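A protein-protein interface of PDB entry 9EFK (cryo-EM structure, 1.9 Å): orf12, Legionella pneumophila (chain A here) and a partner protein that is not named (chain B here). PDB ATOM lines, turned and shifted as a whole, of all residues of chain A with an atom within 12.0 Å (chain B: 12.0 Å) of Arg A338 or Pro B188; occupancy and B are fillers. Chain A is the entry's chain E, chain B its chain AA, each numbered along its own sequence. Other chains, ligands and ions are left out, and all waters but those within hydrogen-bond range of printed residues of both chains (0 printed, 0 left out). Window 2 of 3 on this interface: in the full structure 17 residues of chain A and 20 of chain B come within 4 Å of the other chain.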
ATOM      1  N   ASN A 331     -23.547  13.705 -19.177  1.00  0.00           N
ATOM      2  CA  ASN A 331     -24.591  13.619 -18.163  1.00  0.00           C
ATOM      3  C   ASN A 331     -24.662  12.183 -17.658  1.00  0.00           C
ATOM      4  O   ASN A 331     -25.105  11.288 -18.382  1.00  0.00           O
ATOM      5  CB  ASN A 331     -25.922  14.071 -18.757  1.00  0.00           C
ATOM      6  CG  ASN A 331     -27.002  14.264 -17.720  1.00  0.00           C
ATOM      7  OD1 ASN A 331     -27.006  13.621 -16.679  1.00  0.00           O
ATOM      8  ND2 ASN A 331     -27.939  15.149 -18.012  1.00  0.00           N
ATOM      9  N   GLN A 332     -24.237  11.960 -16.412  1.00  0.00           N
ATOM     10  CA  GLN A 332     -24.250  10.611 -15.854  1.00  0.00           C
ATOM     11  C   GLN A 332     -25.664  10.068 -15.699  1.00  0.00           C
ATOM     12  O   GLN A 332     -25.861   8.852 -15.732  1.00  0.00           O
ATOM     13  CB  GLN A 332     -23.539  10.578 -14.500  1.00  0.00           C
ATOM     14  CG  GLN A 332     -22.025  10.638 -14.564  1.00  0.00           C
ATOM     15  CD  GLN A 332     -21.502  12.034 -14.812  1.00  0.00           C
ATOM     16  OE1 GLN A 332     -22.200  13.018 -14.592  1.00  0.00           O
ATOM     17  NE2 GLN A 332     -20.265  12.126 -15.270  1.00  0.00           N
ATOM     18  N   GLN A 333     -26.652  10.943 -15.513  1.00  0.00           N
ATOM     19  CA  GLN A 333     -28.015  10.493 -15.259  1.00  0.00           C
ATOM     20  C   GLN A 333     -28.719  10.018 -16.519  1.00  0.00           C
ATOM     21  O   GLN A 333     -29.558   9.116 -16.447  1.00  0.00           O
ATOM     22  CB  GLN A 333     -28.828  11.610 -14.615  1.00  0.00           C
ATOM     23  CG  GLN A 333     -28.016  12.511 -13.729  1.00  0.00           C
ATOM     24  CD  GLN A 333     -27.487  11.799 -12.523  1.00  0.00           C
ATOM     25  OE1 GLN A 333     -28.089  10.843 -12.043  1.00  0.00           O
ATOM     26  NE2 GLN A 333     -26.349  12.253 -12.021  1.00  0.00           N
ATOM     27  N   THR A 334     -28.417  10.613 -17.668  1.00  0.00           N
ATOM     28  CA  THR A 334     -29.010  10.189 -18.926  1.00  0.00           C
ATOM     29  C   THR A 334     -28.071   9.332 -19.763  1.00  0.00           C
ATOM     30  O   THR A 334     -28.419   8.988 -20.893  1.00  0.00           O
ATOM     31  CB  THR A 334     -29.466  11.405 -19.739  1.00  0.00           C
ATOM     32  OG1 THR A 334     -28.323  12.141 -20.182  1.00  0.00           O
ATOM     33  CG2 THR A 334     -30.344  12.309 -18.898  1.00  0.00           C
ATOM     34  N   PHE A 335     -26.895   8.994 -19.244  1.00  0.00           N
ATOM     35  CA  PHE A 335     -25.964   8.130 -19.959  1.00  0.00           C
ATOM     36  C   PHE A 335     -26.636   6.803 -20.290  1.00  0.00           C
ATOM     37  O   PHE A 335     -27.234   6.165 -19.421  1.00  0.00           O
ATOM     38  CB  PHE A 335     -24.718   7.906 -19.102  1.00  0.00           C
ATOM     39  CG  PHE A 335     -23.571   7.269 -19.831  1.00  0.00           C
ATOM     40  CD1 PHE A 335     -23.508   5.900 -19.993  1.00  0.00           C
ATOM     41  CD2 PHE A 335     -22.536   8.043 -20.324  1.00  0.00           C
ATOM     42  CE1 PHE A 335     -22.449   5.316 -20.652  1.00  0.00           C
ATOM     43  CE2 PHE A 335     -21.472   7.463 -20.981  1.00  0.00           C
ATOM     44  CZ  PHE A 335     -21.431   6.098 -21.148  1.00  0.00           C
ATOM     45  N   THR A 336     -26.527   6.384 -21.549  1.00  0.00           N
ATOM     46  CA  THR A 336     -27.266   5.236 -22.075  1.00  0.00           C
ATOM     47  C   THR A 336     -26.289   4.214 -22.639  1.00  0.00           C
ATOM     48  O   THR A 336     -25.901   4.296 -23.814  1.00  0.00           O
ATOM     49  CB  THR A 336     -28.263   5.682 -23.140  1.00  0.00           C
ATOM     50  OG1 THR A 336     -29.056   6.756 -22.624  1.00  0.00           O
ATOM     51  CG2 THR A 336     -29.174   4.535 -23.537  1.00  0.00           C
ATOM     52  N   PRO A 337     -25.859   3.238 -21.841  1.00  0.00           N
ATOM     53  CA  PRO A 337     -24.906   2.215 -22.319  1.00  0.00           C
ATOM     54  C   PRO A 337     -25.576   1.081 -23.092  1.00  0.00           C
ATOM     55  O   PRO A 337     -25.824  -0.011 -22.596  1.00  0.00           O
ATOM     56  CB  PRO A 337     -24.265   1.727 -21.019  1.00  0.00           C
ATOM     57  CG  PRO A 337     -25.316   1.917 -19.997  1.00  0.00           C
ATOM     58  CD  PRO A 337     -26.155   3.092 -20.408  1.00  0.00           C
ATOM     59  N   ARG A 338     -25.878   1.352 -24.355  1.00  0.00           N
ATOM     60  CA  ARG A 338     -26.571   0.432 -25.238  1.00  0.00           C
ATOM     61  C   ARG A 338     -25.809   0.305 -26.547  1.00  0.00           C
ATOM     62  O   ARG A 338     -25.156   1.257 -26.978  1.00  0.00           O
ATOM     63  CB  ARG A 338     -27.999   0.925 -25.517  1.00  0.00           C
ATOM     64  CG  ARG A 338     -29.112  -0.066 -25.224  1.00  0.00           C
ATOM     65  CD  ARG A 338     -29.367  -0.244 -23.732  1.00  0.00           C
ATOM     66  NE  ARG A 338     -28.373  -1.113 -23.119  1.00  0.00           N
ATOM     67  CZ  ARG A 338     -28.371  -2.435 -23.208  1.00  0.00           C
ATOM     68  NH1 ARG A 338     -29.337  -3.087 -23.833  1.00  0.00           N
ATOM     69  NH2 ARG A 338     -27.371  -3.120 -22.665  1.00  0.00           N
ATOM     70  N   PRO A 339     -25.866  -0.852 -27.201  1.00  0.00           N
ATOM     71  CA  PRO A 339     -25.185  -0.991 -28.492  1.00  0.00           C
ATOM     72  C   PRO A 339     -25.785  -0.056 -29.531  1.00  0.00           C
ATOM     73  O   PRO A 339     -26.999  -0.011 -29.728  1.00  0.00           O
ATOM     74  CB  PRO A 339     -25.396  -2.465 -28.852  1.00  0.00           C
ATOM     75  CG  PRO A 339     -26.533  -2.908 -28.020  1.00  0.00           C
ATOM     76  CD  PRO A 339     -26.480  -2.115 -26.765  1.00  0.00           C
ATOM     77  N   GLY A 340     -24.918   0.704 -30.189  1.00  0.00           N
ATOM     78  CA  GLY A 340     -25.321   1.700 -31.153  1.00  0.00           C
ATOM     79  C   GLY A 340     -25.682   3.047 -30.575  1.00  0.00           C
ATOM     80  O   GLY A 340     -26.021   3.958 -31.338  1.00  0.00           O
ATOM     81  N   SER A 341     -25.607   3.213 -29.260  1.00  0.00           N
ATOM     82  CA  SER A 341     -26.034   4.456 -28.636  1.00  0.00           C
ATOM     83  C   SER A 341     -25.005   5.560 -28.841  1.00  0.00           C
ATOM     84  O   SER A 341     -23.798   5.326 -28.778  1.00  0.00           O
ATOM     85  CB  SER A 341     -26.274   4.239 -27.145  1.00  0.00           C
ATOM     86  OG  SER A 341     -26.448   5.469 -26.473  1.00  0.00           O
ATOM     87  N   ILE A 342     -25.495   6.772 -29.080  1.00  0.00           N
ATOM     88  CA  ILE A 342     -24.661   7.966 -29.126  1.00  0.00           C
ATOM     89  C   ILE A 342     -24.787   8.688 -27.797  1.00  0.00           C
ATOM     90  O   ILE A 342     -25.897   9.021 -27.367  1.00  0.00           O
ATOM     91  CB  ILE A 342     -25.064   8.901 -30.279  1.00  0.00           C
ATOM     92  CG1 ILE A 342     -24.998   8.189 -31.624  1.00  0.00           C
ATOM     93  CG2 ILE A 342     -24.171  10.122 -30.297  1.00  0.00           C
ATOM     94  CD1 ILE A 342     -25.472   9.057 -32.758  1.00  0.00           C
ATOM     95  N   VAL A 343     -23.661   8.940 -27.150  1.00  0.00           N
ATOM     96  CA  VAL A 343     -23.619   9.693 -25.903  1.00  0.00           C
ATOM     97  C   VAL A 343     -23.190  11.117 -26.232  1.00  0.00           C
ATOM     98  O   VAL A 343     -22.132  11.303 -26.848  1.00  0.00           O
ATOM     99  CB  VAL A 343     -22.668   9.053 -24.884  1.00  0.00           C
ATOM    100  CG1 VAL A 343     -22.666   9.851 -23.597  1.00  0.00           C
ATOM    101  CG2 VAL A 343     -23.087   7.632 -24.618  1.00  0.00           C
ATOM    102  N   PRO A 344     -23.976  12.132 -25.878  1.00  0.00           N
ATOM    103  CA  PRO A 344     -23.506  13.517 -26.015  1.00  0.00           C
ATOM    104  C   PRO A 344     -22.362  13.771 -25.045  1.00  0.00           C
ATOM    105  O   PRO A 344     -22.498  13.554 -23.841  1.00  0.00           O
ATOM    106  CB  PRO A 344     -24.745  14.350 -25.665  1.00  0.00           C
ATOM    107  CG  PRO A 344     -25.889  13.405 -25.750  1.00  0.00           C
ATOM    108  CD  PRO A 344     -25.357  12.070 -25.383  1.00  0.00           C
ATOM    109  N   ASN B  99     -36.397   8.187 -10.798  1.00  0.00           N
ATOM    110  CA  ASN B  99     -35.968   7.767 -12.131  1.00  0.00           C
ATOM    111  C   ASN B  99     -37.170   7.244 -12.914  1.00  0.00           C
ATOM    112  O   ASN B  99     -37.412   6.041 -13.024  1.00  0.00           O
ATOM    113  CB  ASN B  99     -34.871   6.717 -12.017  1.00  0.00           C
ATOM    114  CG  ASN B  99     -34.261   6.367 -13.351  1.00  0.00           C
ATOM    115  OD1 ASN B  99     -34.309   7.154 -14.295  1.00  0.00           O
ATOM    116  ND2 ASN B  99     -33.680   5.179 -13.440  1.00  0.00           N
ATOM    117  N   PRO B 183     -22.622   8.002  -9.972  1.00  0.00           N
ATOM    118  CA  PRO B 183     -22.640   6.847 -10.872  1.00  0.00           C
ATOM    119  C   PRO B 183     -23.694   6.984 -11.961  1.00  0.00           C
ATOM    120  O   PRO B 183     -24.613   7.798 -11.882  1.00  0.00           O
ATOM    121  CB  PRO B 183     -22.978   5.684  -9.935  1.00  0.00           C
ATOM    122  CG  PRO B 183     -23.790   6.317  -8.871  1.00  0.00           C
ATOM    123  CD  PRO B 183     -23.206   7.682  -8.660  1.00  0.00           C
ATOM    124  N   PHE B 184     -23.534   6.161 -12.995  1.00  0.00           N
ATOM    125  CA  PHE B 184     -24.568   6.027 -14.011  1.00  0.00           C
ATOM    126  C   PHE B 184     -25.845   5.483 -13.383  1.00  0.00           C
ATOM    127  O   PHE B 184     -25.804   4.636 -12.491  1.00  0.00           O
ATOM    128  CB  PHE B 184     -24.113   5.084 -15.126  1.00  0.00           C
ATOM    129  CG  PHE B 184     -22.912   5.561 -15.885  1.00  0.00           C
ATOM    130  CD1 PHE B 184     -22.619   6.905 -15.985  1.00  0.00           C
ATOM    131  CD2 PHE B 184     -22.082   4.654 -16.515  1.00  0.00           C
ATOM    132  CE1 PHE B 184     -21.519   7.334 -16.687  1.00  0.00           C
ATOM    133  CE2 PHE B 184     -20.982   5.079 -17.222  1.00  0.00           C
ATOM    134  CZ  PHE B 184     -20.700   6.421 -17.306  1.00  0.00           C
ATOM    135  N   ARG B 185     -26.988   5.980 -13.848  1.00  0.00           N
ATOM    136  CA  ARG B 185     -28.263   5.468 -13.368  1.00  0.00           C
ATOM    137  C   ARG B 185     -28.737   4.236 -14.120  1.00  0.00           C
ATOM    138  O   ARG B 185     -29.648   3.554 -13.644  1.00  0.00           O
ATOM    139  CB  ARG B 185     -29.339   6.553 -13.448  1.00  0.00           C
ATOM    140  CG  ARG B 185     -29.087   7.713 -12.513  1.00  0.00           C
ATOM    141  CD  ARG B 185     -30.376   8.268 -11.931  1.00  0.00           C
ATOM    142  NE  ARG B 185     -31.216   8.903 -12.937  1.00  0.00           N
ATOM    143  CZ  ARG B 185     -32.285   9.636 -12.661  1.00  0.00           C
ATOM    144  NH1 ARG B 185     -32.678   9.841 -11.416  1.00  0.00           N
ATOM    145  NH2 ARG B 185     -32.973  10.182 -13.659  1.00  0.00           N
ATOM    146  N   HIS B 186     -28.144   3.928 -15.268  1.00  0.00           N
ATOM    147  CA  HIS B 186     -28.516   2.762 -16.056  1.00  0.00           C
ATOM    148  C   HIS B 186     -27.297   1.864 -16.198  1.00  0.00           C
ATOM    149  O   HIS B 186     -26.282   2.278 -16.763  1.00  0.00           O
ATOM    150  CB  HIS B 186     -29.053   3.177 -17.427  1.00  0.00           C
ATOM    151  CG  HIS B 186     -30.149   4.195 -17.358  1.00  0.00           C
ATOM    152  ND1 HIS B 186     -29.921   5.545 -17.517  1.00  0.00           N
ATOM    153  CD2 HIS B 186     -31.476   4.063 -17.133  1.00  0.00           C
ATOM    154  CE1 HIS B 186     -31.063   6.199 -17.402  1.00  0.00           C
ATOM    155  NE2 HIS B 186     -32.023   5.323 -17.168  1.00  0.00           N
ATOM    156  N   ASN B 187     -27.395   0.644 -15.675  1.00  0.00           N
ATOM    157  CA  ASN B 187     -26.313  -0.339 -15.740  1.00  0.00           C
ATOM    158  C   ASN B 187     -26.904  -1.674 -16.161  1.00  0.00           C
ATOM    159  O   ASN B 187     -27.203  -2.530 -15.324  1.00  0.00           O
ATOM    160  CB  ASN B 187     -25.589  -0.447 -14.396  1.00  0.00           C
ATOM    161  CG  ASN B 187     -25.003   0.876 -13.939  1.00  0.00           C
ATOM    162  OD1 ASN B 187     -23.935   1.280 -14.387  1.00  0.00           O
ATOM    163  ND2 ASN B 187     -25.702   1.555 -13.043  1.00  0.00           N
ATOM    164  N   PRO B 188     -27.068  -1.893 -17.470  1.00  0.00           N
ATOM    165  CA  PRO B 188     -27.917  -3.006 -17.935  1.00  0.00           C
ATOM    166  C   PRO B 188     -27.491  -4.390 -17.476  1.00  0.00           C
ATOM    167  O   PRO B 188     -28.354  -5.200 -17.123  1.00  0.00           O
ATOM    168  CB  PRO B 188     -27.830  -2.881 -19.461  1.00  0.00           C
ATOM    169  CG  PRO B 188     -27.434  -1.478 -19.708  1.00  0.00           C
ATOM    170  CD  PRO B 188     -26.535  -1.104 -18.587  1.00  0.00           C
ATOM    171  N   TYR B 189     -26.194  -4.700 -17.469  1.00  0.00           N
ATOM    172  CA  TYR B 189     -25.781  -6.053 -17.117  1.00  0.00           C
ATOM    173  C   TYR B 189     -25.961  -6.351 -15.638  1.00  0.00           C
ATOM    174  O   TYR B 189     -25.920  -7.520 -15.251  1.00  0.00           O
ATOM    175  CB  TYR B 189     -24.328  -6.300 -17.515  1.00  0.00           C
ATOM    176  CG  TYR B 189     -24.084  -6.278 -19.002  1.00  0.00           C
ATOM    177  CD1 TYR B 189     -25.137  -6.255 -19.902  1.00  0.00           C
ATOM    178  CD2 TYR B 189     -22.798  -6.289 -19.507  1.00  0.00           C
ATOM    179  CE1 TYR B 189     -24.911  -6.230 -21.257  1.00  0.00           C
ATOM    180  CE2 TYR B 189     -22.564  -6.267 -20.861  1.00  0.00           C
ATOM    181  CZ  TYR B 189     -23.622  -6.236 -21.730  1.00  0.00           C
ATOM    182  OH  TYR B 189     -23.383  -6.217 -23.079  1.00  0.00           O
ATOM    183  N   VAL B 190     -26.155  -5.326 -14.817  1.00  0.00           N
ATOM    184  CA  VAL B 190     -26.466  -5.493 -13.408  1.00  0.00           C
ATOM    185  C   VAL B 190     -27.962  -5.388 -13.151  1.00  0.00           C
ATOM    186  O   VAL B 190     -28.520  -6.173 -12.387  1.00  0.00           O
ATOM    187  CB  VAL B 190     -25.689  -4.452 -12.574  1.00  0.00           C
ATOM    188  CG1 VAL B 190     -26.048  -4.568 -11.107  1.00  0.00           C
ATOM    189  CG2 VAL B 190     -24.201  -4.612 -12.779  1.00  0.00           C
ATOM    190  N   ASP B 191     -28.622  -4.420 -13.790  1.00  0.00           N
ATOM    191  CA  ASP B 191     -30.045  -4.199 -13.558  1.00  0.00           C
ATOM    192  C   ASP B 191     -30.882  -5.389 -13.994  1.00  0.00           C
ATOM    193  O   ASP B 191     -31.946  -5.637 -13.420  1.00  0.00           O
ATOM    194  CB  ASP B 191     -30.509  -2.941 -14.294  1.00  0.00           C
ATOM    195  CG  ASP B 191     -29.796  -1.687 -13.825  1.00  0.00           C
ATOM    196  OD1 ASP B 191     -29.099  -1.736 -12.792  1.00  0.00           O
ATOM    197  OD2 ASP B 191     -29.932  -0.645 -14.498  1.00  0.00           O
ATOM    198  N   VAL B 192     -30.427  -6.132 -15.006  1.00  0.00           N
ATOM    199  CA  VAL B 192     -31.199  -7.256 -15.518  1.00  0.00           C
ATOM    200  C   VAL B 192     -31.375  -8.340 -14.466  1.00  0.00           C
ATOM    201  O   VAL B 192     -32.337  -9.111 -14.529  1.00  0.00           O
ATOM    202  CB  VAL B 192     -30.539  -7.811 -16.799  1.00  0.00           C
ATOM    203  CG1 VAL B 192     -29.258  -8.551 -16.478  1.00  0.00           C
ATOM    204  CG2 VAL B 192     -31.501  -8.700 -17.555  1.00  0.00           C
ATOM    205  N   ARG B 193     -30.477  -8.416 -13.493  1.00  0.00           N
ATOM    206  CA  ARG B 193     -30.598  -9.387 -12.416  1.00  0.00           C
ATOM    207  C   ARG B 193     -31.773  -9.056 -11.509  1.00  0.00           C
ATOM    208  O   ARG B 193     -32.167  -9.868 -10.680  1.00  0.00           O
ATOM    209  CB  ARG B 193     -29.315  -9.439 -11.601  1.00  0.00           C
ATOM    210  CG  ARG B 193     -28.093  -9.762 -12.413  1.00  0.00           C
ATOM    211  CD  ARG B 193     -26.841  -9.617 -11.585  1.00  0.00           C
ATOM    212  NE  ARG B 193     -25.794 -10.499 -12.075  1.00  0.00           N
ATOM    213  CZ  ARG B 193     -25.385 -11.595 -11.458  1.00  0.00           C
ATOM    214  NH1 ARG B 193     -25.846 -11.931 -10.268  1.00  0.00           N
ATOM    215  NH2 ARG B 193     -24.483 -12.371 -12.047  1.00  0.00           N
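Of the printed residues of chain B, Gln A332 touches Pro B183, Phe B184 and Arg B185. Of the printed residues of chain B, Gln A333 touches Arg B185 (3.3 Å) and His B186 (3.4 Å). Thr A334 touches none of the printed residues of chain B. No residue of chain B comes within 4 Å of Thr A336. Pro A337 touches two residues of chain B. Arg A338 touches just one residue of chain B: Pro B188. No residue of chain B comes within 4 Å of Pro A339. No residue of chain B comes within 4 Å of Gly A340. Asn B99 touches none of the printed residues of chain A. Of the printed residues of chain A, Pro B183 touches Gln A332 (3.97 Å). Of the printed residues of chain A, Phe B184 touches Gln A332 (3.6 Å) and Phe A335 (3.7 Å). Printed residues of chain A within 4 Å of His B186: Gln A333, Phe A335 and Pro A337. No residue of chain A comes within 4 Å of Tyr B189. No residue of chain A comes within 4 Å of Val B190. No residue of chain A comes within 4 Å of Asp B191. The nearest residue of chain B that does not touch Arg A338 is Tyr B189 (4.2 Å). The nearest printed residue of chain A that does not touch His B186 is Thr A334 (4.7 Å).
Gln A332 touches Pro B183 (CB to O, 3.97 Å). Phe B184 touches Gln A332. Arg B185 touches Gln A332. Arg B185 touches Gln A333 (CG to OE1, 3.3 Å). Gln A333 touches His B186. Phe A335 touches Phe B184. Pro A337 touches His B186 (CG to O, 3.4 Å). Pro A337 touches Pro B188. Pro B188 touches Arg A338 (CB to NH2, 3.2 Å).
Printed residues of chain B that touch a printed residue of chain A: Pro B183, Phe B184, Arg B185, His B186 and Pro B188. Hydrophobic or aromatic side chains of chain B that line the printed part of chain A: Phe B184, His B186 and Pro B188. Printed residues of chain A that touch a printed residue of chain B: Gln A332, Gln A333, Phe A335, Pro A337 and Arg A338. Hydrophobic or aromatic side chains of chain A that line the printed part of chain B: Phe A335 and Pro A337. Among the printed residues, 10 pairs touch across the chains. Among the printed residues, no Asp or Glu carboxylate lies within 4 Å of a Lys or Arg side-chain nitrogen of the other chain.
ND1 of His B186 lies within hydrogen-bond range of O of Phe A335.
The side-chain amide oxygen of Asn A331 is in hydrogen-bond range of the backbone NH of Gln A333, at 2.9 Å. ND2 of Asn B187 lies within hydrogen-bond range of O of Phe B184, 3.1 Å away. The guanidinium group (NH2) of Arg B185 lies within hydrogen-bond range of the side-chain amide oxygen (OD1) of Asn B99 (3.4 Å).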
